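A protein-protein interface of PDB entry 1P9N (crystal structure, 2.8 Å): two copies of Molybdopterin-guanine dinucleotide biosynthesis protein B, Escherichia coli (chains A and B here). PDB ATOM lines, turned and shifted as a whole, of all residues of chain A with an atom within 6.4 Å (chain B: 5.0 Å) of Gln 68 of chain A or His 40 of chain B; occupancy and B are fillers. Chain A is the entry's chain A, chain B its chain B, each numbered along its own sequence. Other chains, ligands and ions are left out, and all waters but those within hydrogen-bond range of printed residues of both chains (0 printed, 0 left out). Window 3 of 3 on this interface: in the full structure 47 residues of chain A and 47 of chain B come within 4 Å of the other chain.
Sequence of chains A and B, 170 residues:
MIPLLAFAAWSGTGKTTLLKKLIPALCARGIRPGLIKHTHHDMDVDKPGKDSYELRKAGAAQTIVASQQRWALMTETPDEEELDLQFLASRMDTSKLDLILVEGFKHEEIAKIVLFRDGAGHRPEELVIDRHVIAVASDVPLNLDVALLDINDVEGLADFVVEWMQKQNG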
ATOM      1  N   ALA A  66       9.469  33.541 -10.663  1.00  0.00           N
ATOM      2  CA  ALA A  66      10.304  33.258  -9.497  1.00  0.00           C
ATOM      3  C   ALA A  66      10.471  31.760  -9.280  1.00  0.00           C
ATOM      4  O   ALA A  66       9.862  30.933  -9.967  1.00  0.00           O
ATOM      5  CB  ALA A  66       9.723  33.898  -8.245  1.00  0.00           C
ATOM      6  N   SER A  67      11.308  31.421  -8.311  1.00  0.00           N
ATOM      7  CA  SER A  67      11.596  30.034  -8.003  1.00  0.00           C
ATOM      8  C   SER A  67      12.327  30.014  -6.667  1.00  0.00           C
ATOM      9  O   SER A  67      12.159  30.921  -5.849  1.00  0.00           O
ATOM     10  CB  SER A  67      12.466  29.441  -9.113  1.00  0.00           C
ATOM     11  OG  SER A  67      12.511  28.033  -9.034  1.00  0.00           O
ATOM     12  N   GLN A  68      13.136  28.987  -6.440  1.00  0.00           N
ATOM     13  CA  GLN A  68      13.877  28.878  -5.185  1.00  0.00           C
ATOM     14  C   GLN A  68      15.359  29.157  -5.431  1.00  0.00           C
ATOM     15  O   GLN A  68      16.016  29.835  -4.636  1.00  0.00           O
ATOM     16  CB  GLN A  68      13.715  27.474  -4.588  1.00  0.00           C
ATOM     17  CG  GLN A  68      12.289  26.910  -4.597  1.00  0.00           C
ATOM     18  CD  GLN A  68      11.848  26.406  -5.966  1.00  0.00           C
ATOM     19  OE1 GLN A  68      12.596  25.714  -6.664  1.00  0.00           O
ATOM     20  NE2 GLN A  68      10.622  26.738  -6.348  1.00  0.00           N
ATOM     21  N   GLN A  69      15.865  28.629  -6.545  1.00  0.00           N
ATOM     22  CA  GLN A  69      17.263  28.781  -6.951  1.00  0.00           C
ATOM     23  C   GLN A  69      17.558  30.122  -7.647  1.00  0.00           C
ATOM     24  O   GLN A  69      18.644  30.678  -7.499  1.00  0.00           O
ATOM     25  CB  GLN A  69      17.651  27.631  -7.889  1.00  0.00           C
ATOM     26  CG  GLN A  69      17.466  26.223  -7.320  1.00  0.00           C
ATOM     27  CD  GLN A  69      18.392  25.917  -6.147  1.00  0.00           C
ATOM     28  OE1 GLN A  69      18.060  26.174  -4.988  1.00  0.00           O
ATOM     29  NE2 GLN A  69      19.568  25.373  -6.453  1.00  0.00           N
ATOM     30  N   ARG A  70      16.592  30.617  -8.420  1.00  0.00           N
ATOM     31  CA  ARG A  70      16.727  31.883  -9.143  1.00  0.00           C
ATOM     32  C   ARG A  70      15.418  32.365  -9.766  1.00  0.00           C
ATOM     33  O   ARG A  70      14.420  31.646  -9.763  1.00  0.00           O
ATOM     34  CB  ARG A  70      17.778  31.773 -10.250  1.00  0.00           C
ATOM     35  CG  ARG A  70      18.022  30.375 -10.799  1.00  0.00           C
ATOM     36  CD  ARG A  70      16.764  29.600 -11.124  1.00  0.00           C
ATOM     37  NE  ARG A  70      17.082  28.400 -11.896  1.00  0.00           N
ATOM     38  CZ  ARG A  70      18.067  27.550 -11.608  1.00  0.00           C
ATOM     39  NH1 ARG A  70      18.849  27.753 -10.557  1.00  0.00           N
ATOM     40  NH2 ARG A  70      18.278  26.493 -12.381  1.00  0.00           N
ATOM     41  N   HIS B  38       4.928  32.276  -9.586  1.00  0.00           N
ATOM     42  CA  HIS B  38       5.804  31.469  -8.748  1.00  0.00           C
ATOM     43  C   HIS B  38       5.568  30.011  -9.113  1.00  0.00           C
ATOM     44  O   HIS B  38       4.441  29.532  -9.044  1.00  0.00           O
ATOM     45  CB  HIS B  38       5.455  31.708  -7.282  1.00  0.00           C
ATOM     46  CG  HIS B  38       6.366  31.013  -6.324  1.00  0.00           C
ATOM     47  ND1 HIS B  38       6.911  29.773  -6.585  1.00  0.00           N
ATOM     48  CD2 HIS B  38       6.800  31.367  -5.092  1.00  0.00           C
ATOM     49  CE1 HIS B  38       7.642  29.395  -5.552  1.00  0.00           C
ATOM     50  NE2 HIS B  38       7.591  30.344  -4.632  1.00  0.00           N
ATOM     51  N   THR B  39       6.618  29.305  -9.512  1.00  0.00           N
ATOM     52  CA  THR B  39       6.462  27.909  -9.887  1.00  0.00           C
ATOM     53  C   THR B  39       7.230  27.004  -8.939  1.00  0.00           C
ATOM     54  O   THR B  39       7.606  27.418  -7.839  1.00  0.00           O
ATOM     55  CB  THR B  39       6.952  27.653 -11.331  1.00  0.00           C
ATOM     56  OG1 THR B  39       6.759  26.274 -11.672  1.00  0.00           O
ATOM     57  CG2 THR B  39       8.420  28.003 -11.458  1.00  0.00           C
ATOM     58  N   HIS B  40       7.441  25.765  -9.377  1.00  0.00           N
ATOM     59  CA  HIS B  40       8.175  24.756  -8.621  1.00  0.00           C
ATOM     60  C   HIS B  40       9.038  23.964  -9.594  1.00  0.00           C
ATOM     61  O   HIS B  40      10.092  23.445  -9.225  1.00  0.00           O
ATOM     62  CB  HIS B  40       7.213  23.788  -7.919  1.00  0.00           C
ATOM     63  CG  HIS B  40       6.966  24.108  -6.478  1.00  0.00           C
ATOM     64  ND1 HIS B  40       6.240  25.207  -6.070  1.00  0.00           N
ATOM     65  CD2 HIS B  40       7.354  23.474  -5.346  1.00  0.00           C
ATOM     66  CE1 HIS B  40       6.192  25.237  -4.750  1.00  0.00           C
ATOM     67  NE2 HIS B  40       6.862  24.196  -4.286  1.00  0.00           N
ATOM     68  N   HIS B  41       8.580  23.897 -10.843  1.00  0.00           N
ATOM     69  CA  HIS B  41       9.252  23.152 -11.908  1.00  0.00           C
ATOM     70  C   HIS B  41      10.553  23.772 -12.454  1.00  0.00           C
ATOM     71  O   HIS B  41      11.072  23.312 -13.472  1.00  0.00           O
ATOM     72  CB  HIS B  41       8.260  22.938 -13.060  1.00  0.00           C
ATOM     73  CG  HIS B  41       8.426  21.632 -13.777  1.00  0.00           C
ATOM     74  ND1 HIS B  41       9.602  21.258 -14.390  1.00  0.00           N
ATOM     75  CD2 HIS B  41       7.551  20.619 -13.992  1.00  0.00           C
ATOM     76  CE1 HIS B  41       9.447  20.073 -14.952  1.00  0.00           C
ATOM     77  NE2 HIS B  41       8.211  19.664 -14.726  1.00  0.00           N
ATOM     78  N   ASP B  42      11.069  24.799 -11.777  1.00  0.00           N
ATOM     79  CA  ASP B  42      12.308  25.495 -12.172  1.00  0.00           C
ATOM     80  C   ASP B  42      12.576  25.653 -13.674  1.00  0.00           C
ATOM     81  O   ASP B  42      12.697  24.668 -14.405  1.00  0.00           O
ATOM     82  CB  ASP B  42      13.527  24.826 -11.526  1.00  0.00           C
ATOM     83  CG  ASP B  42      14.165  25.691 -10.455  1.00  0.00           C
ATOM     84  OD1 ASP B  42      13.529  25.894  -9.401  1.00  0.00           O
ATOM     85  OD2 ASP B  42      15.300  26.171 -10.672  1.00  0.00           O
ATOM     86  N   THR B  77      20.041  32.563  -7.174  1.00  0.00           N
ATOM     87  CA  THR B  77      19.895  32.712  -5.733  1.00  0.00           C
ATOM     88  C   THR B  77      19.963  31.398  -4.956  1.00  0.00           C
ATOM     89  O   THR B  77      19.034  31.075  -4.213  1.00  0.00           O
ATOM     90  CB  THR B  77      18.562  33.403  -5.352  1.00  0.00           C
ATOM     91  OG1 THR B  77      17.516  32.930  -6.209  1.00  0.00           O
ATOM     92  CG2 THR B  77      18.685  34.909  -5.452  1.00  0.00           C
ATOM     93  N   GLU B  80      18.900  30.748  -0.659  1.00  0.00           N
ATOM     94  CA  GLU B  80      17.865  29.994   0.059  1.00  0.00           C
ATOM     95  C   GLU B  80      16.518  30.682  -0.146  1.00  0.00           C
ATOM     96  O   GLU B  80      15.524  30.335   0.497  1.00  0.00           O
ATOM     97  CB  GLU B  80      18.161  29.987   1.567  1.00  0.00           C
ATOM     98  CG  GLU B  80      18.327  31.397   2.216  1.00  0.00           C
ATOM     99  CD  GLU B  80      17.064  32.280   2.172  1.00  0.00           C
ATOM    100  OE1 GLU B  80      15.961  31.795   2.507  1.00  0.00           O
ATOM    101  OE2 GLU B  80      17.178  33.474   1.820  1.00  0.00           O
ATOM    102  N   GLU B  81      16.482  31.633  -1.070  1.00  0.00           N
ATOM    103  CA  GLU B  81      15.291  32.449  -1.259  1.00  0.00           C
ATOM    104  C   GLU B  81      14.474  32.509  -2.547  1.00  0.00           C
ATOM    105  O   GLU B  81      14.317  31.534  -3.295  1.00  0.00           O
ATOM    106  CB  GLU B  81      15.668  33.886  -0.881  1.00  0.00           C
ATOM    107  CG  GLU B  81      17.171  34.148  -1.012  1.00  0.00           C
ATOM    108  CD  GLU B  81      17.501  35.509  -1.577  1.00  0.00           C
ATOM    109  OE1 GLU B  81      16.943  36.513  -1.080  1.00  0.00           O
ATOM    110  OE2 GLU B  81      18.330  35.568  -2.515  1.00  0.00           O
ATOM    111  N   GLU B  82      13.943  33.722  -2.724  1.00  0.00           N
ATOM    112  CA  GLU B  82      13.093  34.196  -3.814  1.00  0.00           C
ATOM    113  C   GLU B  82      11.626  33.821  -3.731  1.00  0.00           C
ATOM    114  O   GLU B  82      11.103  32.988  -4.479  1.00  0.00           O
ATOM    115  CB  GLU B  82      13.707  33.868  -5.173  1.00  0.00           C
ATOM    116  CG  GLU B  82      14.813  34.870  -5.504  1.00  0.00           C
ATOM    117  CD  GLU B  82      14.707  36.177  -4.681  1.00  0.00           C
ATOM    118  OE1 GLU B  82      13.598  36.744  -4.563  1.00  0.00           O
ATOM    119  OE2 GLU B  82      15.739  36.646  -4.150  1.00  0.00           O
ATOM    120  N   LYS B 106       1.873  31.404  -2.162  1.00  0.00           N
ATOM    121  CA  LYS B 106       0.880  31.030  -1.158  1.00  0.00           C
ATOM    122  C   LYS B 106       1.178  31.728   0.169  1.00  0.00           C
ATOM    123  O   LYS B 106       2.338  31.952   0.516  1.00  0.00           O
ATOM    124  CB  LYS B 106       0.874  29.506  -0.938  1.00  0.00           C
ATOM    125  CG  LYS B 106       1.563  28.673  -2.030  1.00  0.00           C
ATOM    126  CD  LYS B 106       3.090  28.793  -1.950  1.00  0.00           C
ATOM    127  CE  LYS B 106       3.806  27.879  -2.947  1.00  0.00           C
ATOM    128  NZ  LYS B 106       3.585  28.264  -4.369  1.00  0.00           N
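Of the 5 printed residues of chain A, 5 touch a printed residue of chain B. Along chain A the printed residues that touch a printed residue of chain B span positions 66 to 70. Among the printed residues, Asp or Glu carboxylates within 4 Å of a Lys or Arg side-chain nitrogen of the other chain: Arg 70 of chain A with Asp 42 of chain B.
The side-chain carboxylate (OD1) of Asp 42 of chain B sits close to the side-chain hydroxyl (OG) of Ser 67 of chain A (2.4 Å). O of Gln 68 of chain A sits close to O of Thr 77 of chain B. OD2 of Asp 42 of chain B lies within salt-bridge range of NE of Arg 70 of chain A (3.1 Å). The backbone carbonyl oxygen (O) of Gln 69 of chain A sits at hydrogen-bond distance from the side-chain hydroxyl (OG1) of Thr 77 of chain B (2.8 Å). O of Glu 81 of chain B sits close to O of Ser 67 of chain A (3.4 Å). The side-chain carboxylate (OD1) of Asp 42 of chain B lies close to the side-chain amide oxygen (OE1) of Gln 68 of chain A, 2.9 Å away. The backbone carbonyl oxygen of Gln 68 of chain A lies close to the backbone carbonyl oxygen of Glu 81 of chain B (2.8 Å). The backbone carbonyl oxygen (O) of Glu 82 of chain B sits close to the backbone carbonyl oxygen (O) of Ser 67 of chain A. The side-chain hydroxyl (OG1) of Thr 77 of chain B sits close to the backbone NH (N) of Arg 70 of chain A (3.3 Å). The side-chain amide nitrogen of Gln 68 of chain A sits at hydrogen-bond distance from the backbone carbonyl oxygen of Thr 39 of chain B.
Gln 68 of chain A touches five residues of chain B. His 40 of chain B touches just one residue of chain A: Gln 68. Printed residues of chain A within 4 Å of Thr 39 of chain B: Ala 66 (3.6 Å) and Gln 68 (3.4 Å). Printed residues of chain B within 4 Å of Ser 67 of chain A: Asp 42, Glu 81 and Glu 82. Lys 106 of chain B touches none of the printed residues of chain A. The nearest residue of chain B that does not touch Gln 68 of chain A is His 38 of chain B (4.1 Å). The nearest printed residue of chain A that does not touch Glu 82 of chain B is Ala 66 of chain A (4.1 Å).
Thr 39 of chain B touches Ala 66 of chain A. Gln 68 of chain A touches His 40 of chain B (NE2 to CA, 3.9 Å). Gln 69 of chain A touches Asp 42 of chain B (CB to OD2, 3.9 Å).
No position is printed for both chains. Of the 13 pairs that touch across the chains among the printed residues, none has its exchanged pair printed and touching as well.
OE1 of Gln 68 of chain A lies within hydrogen-bond range of OG of Ser 67 of chain A, 3.3 Å away. The side-chain hydroxyl of Thr 39 of chain B sits at hydrogen-bond distance from the backbone NH of His 41 of chain B (3.1 Å).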
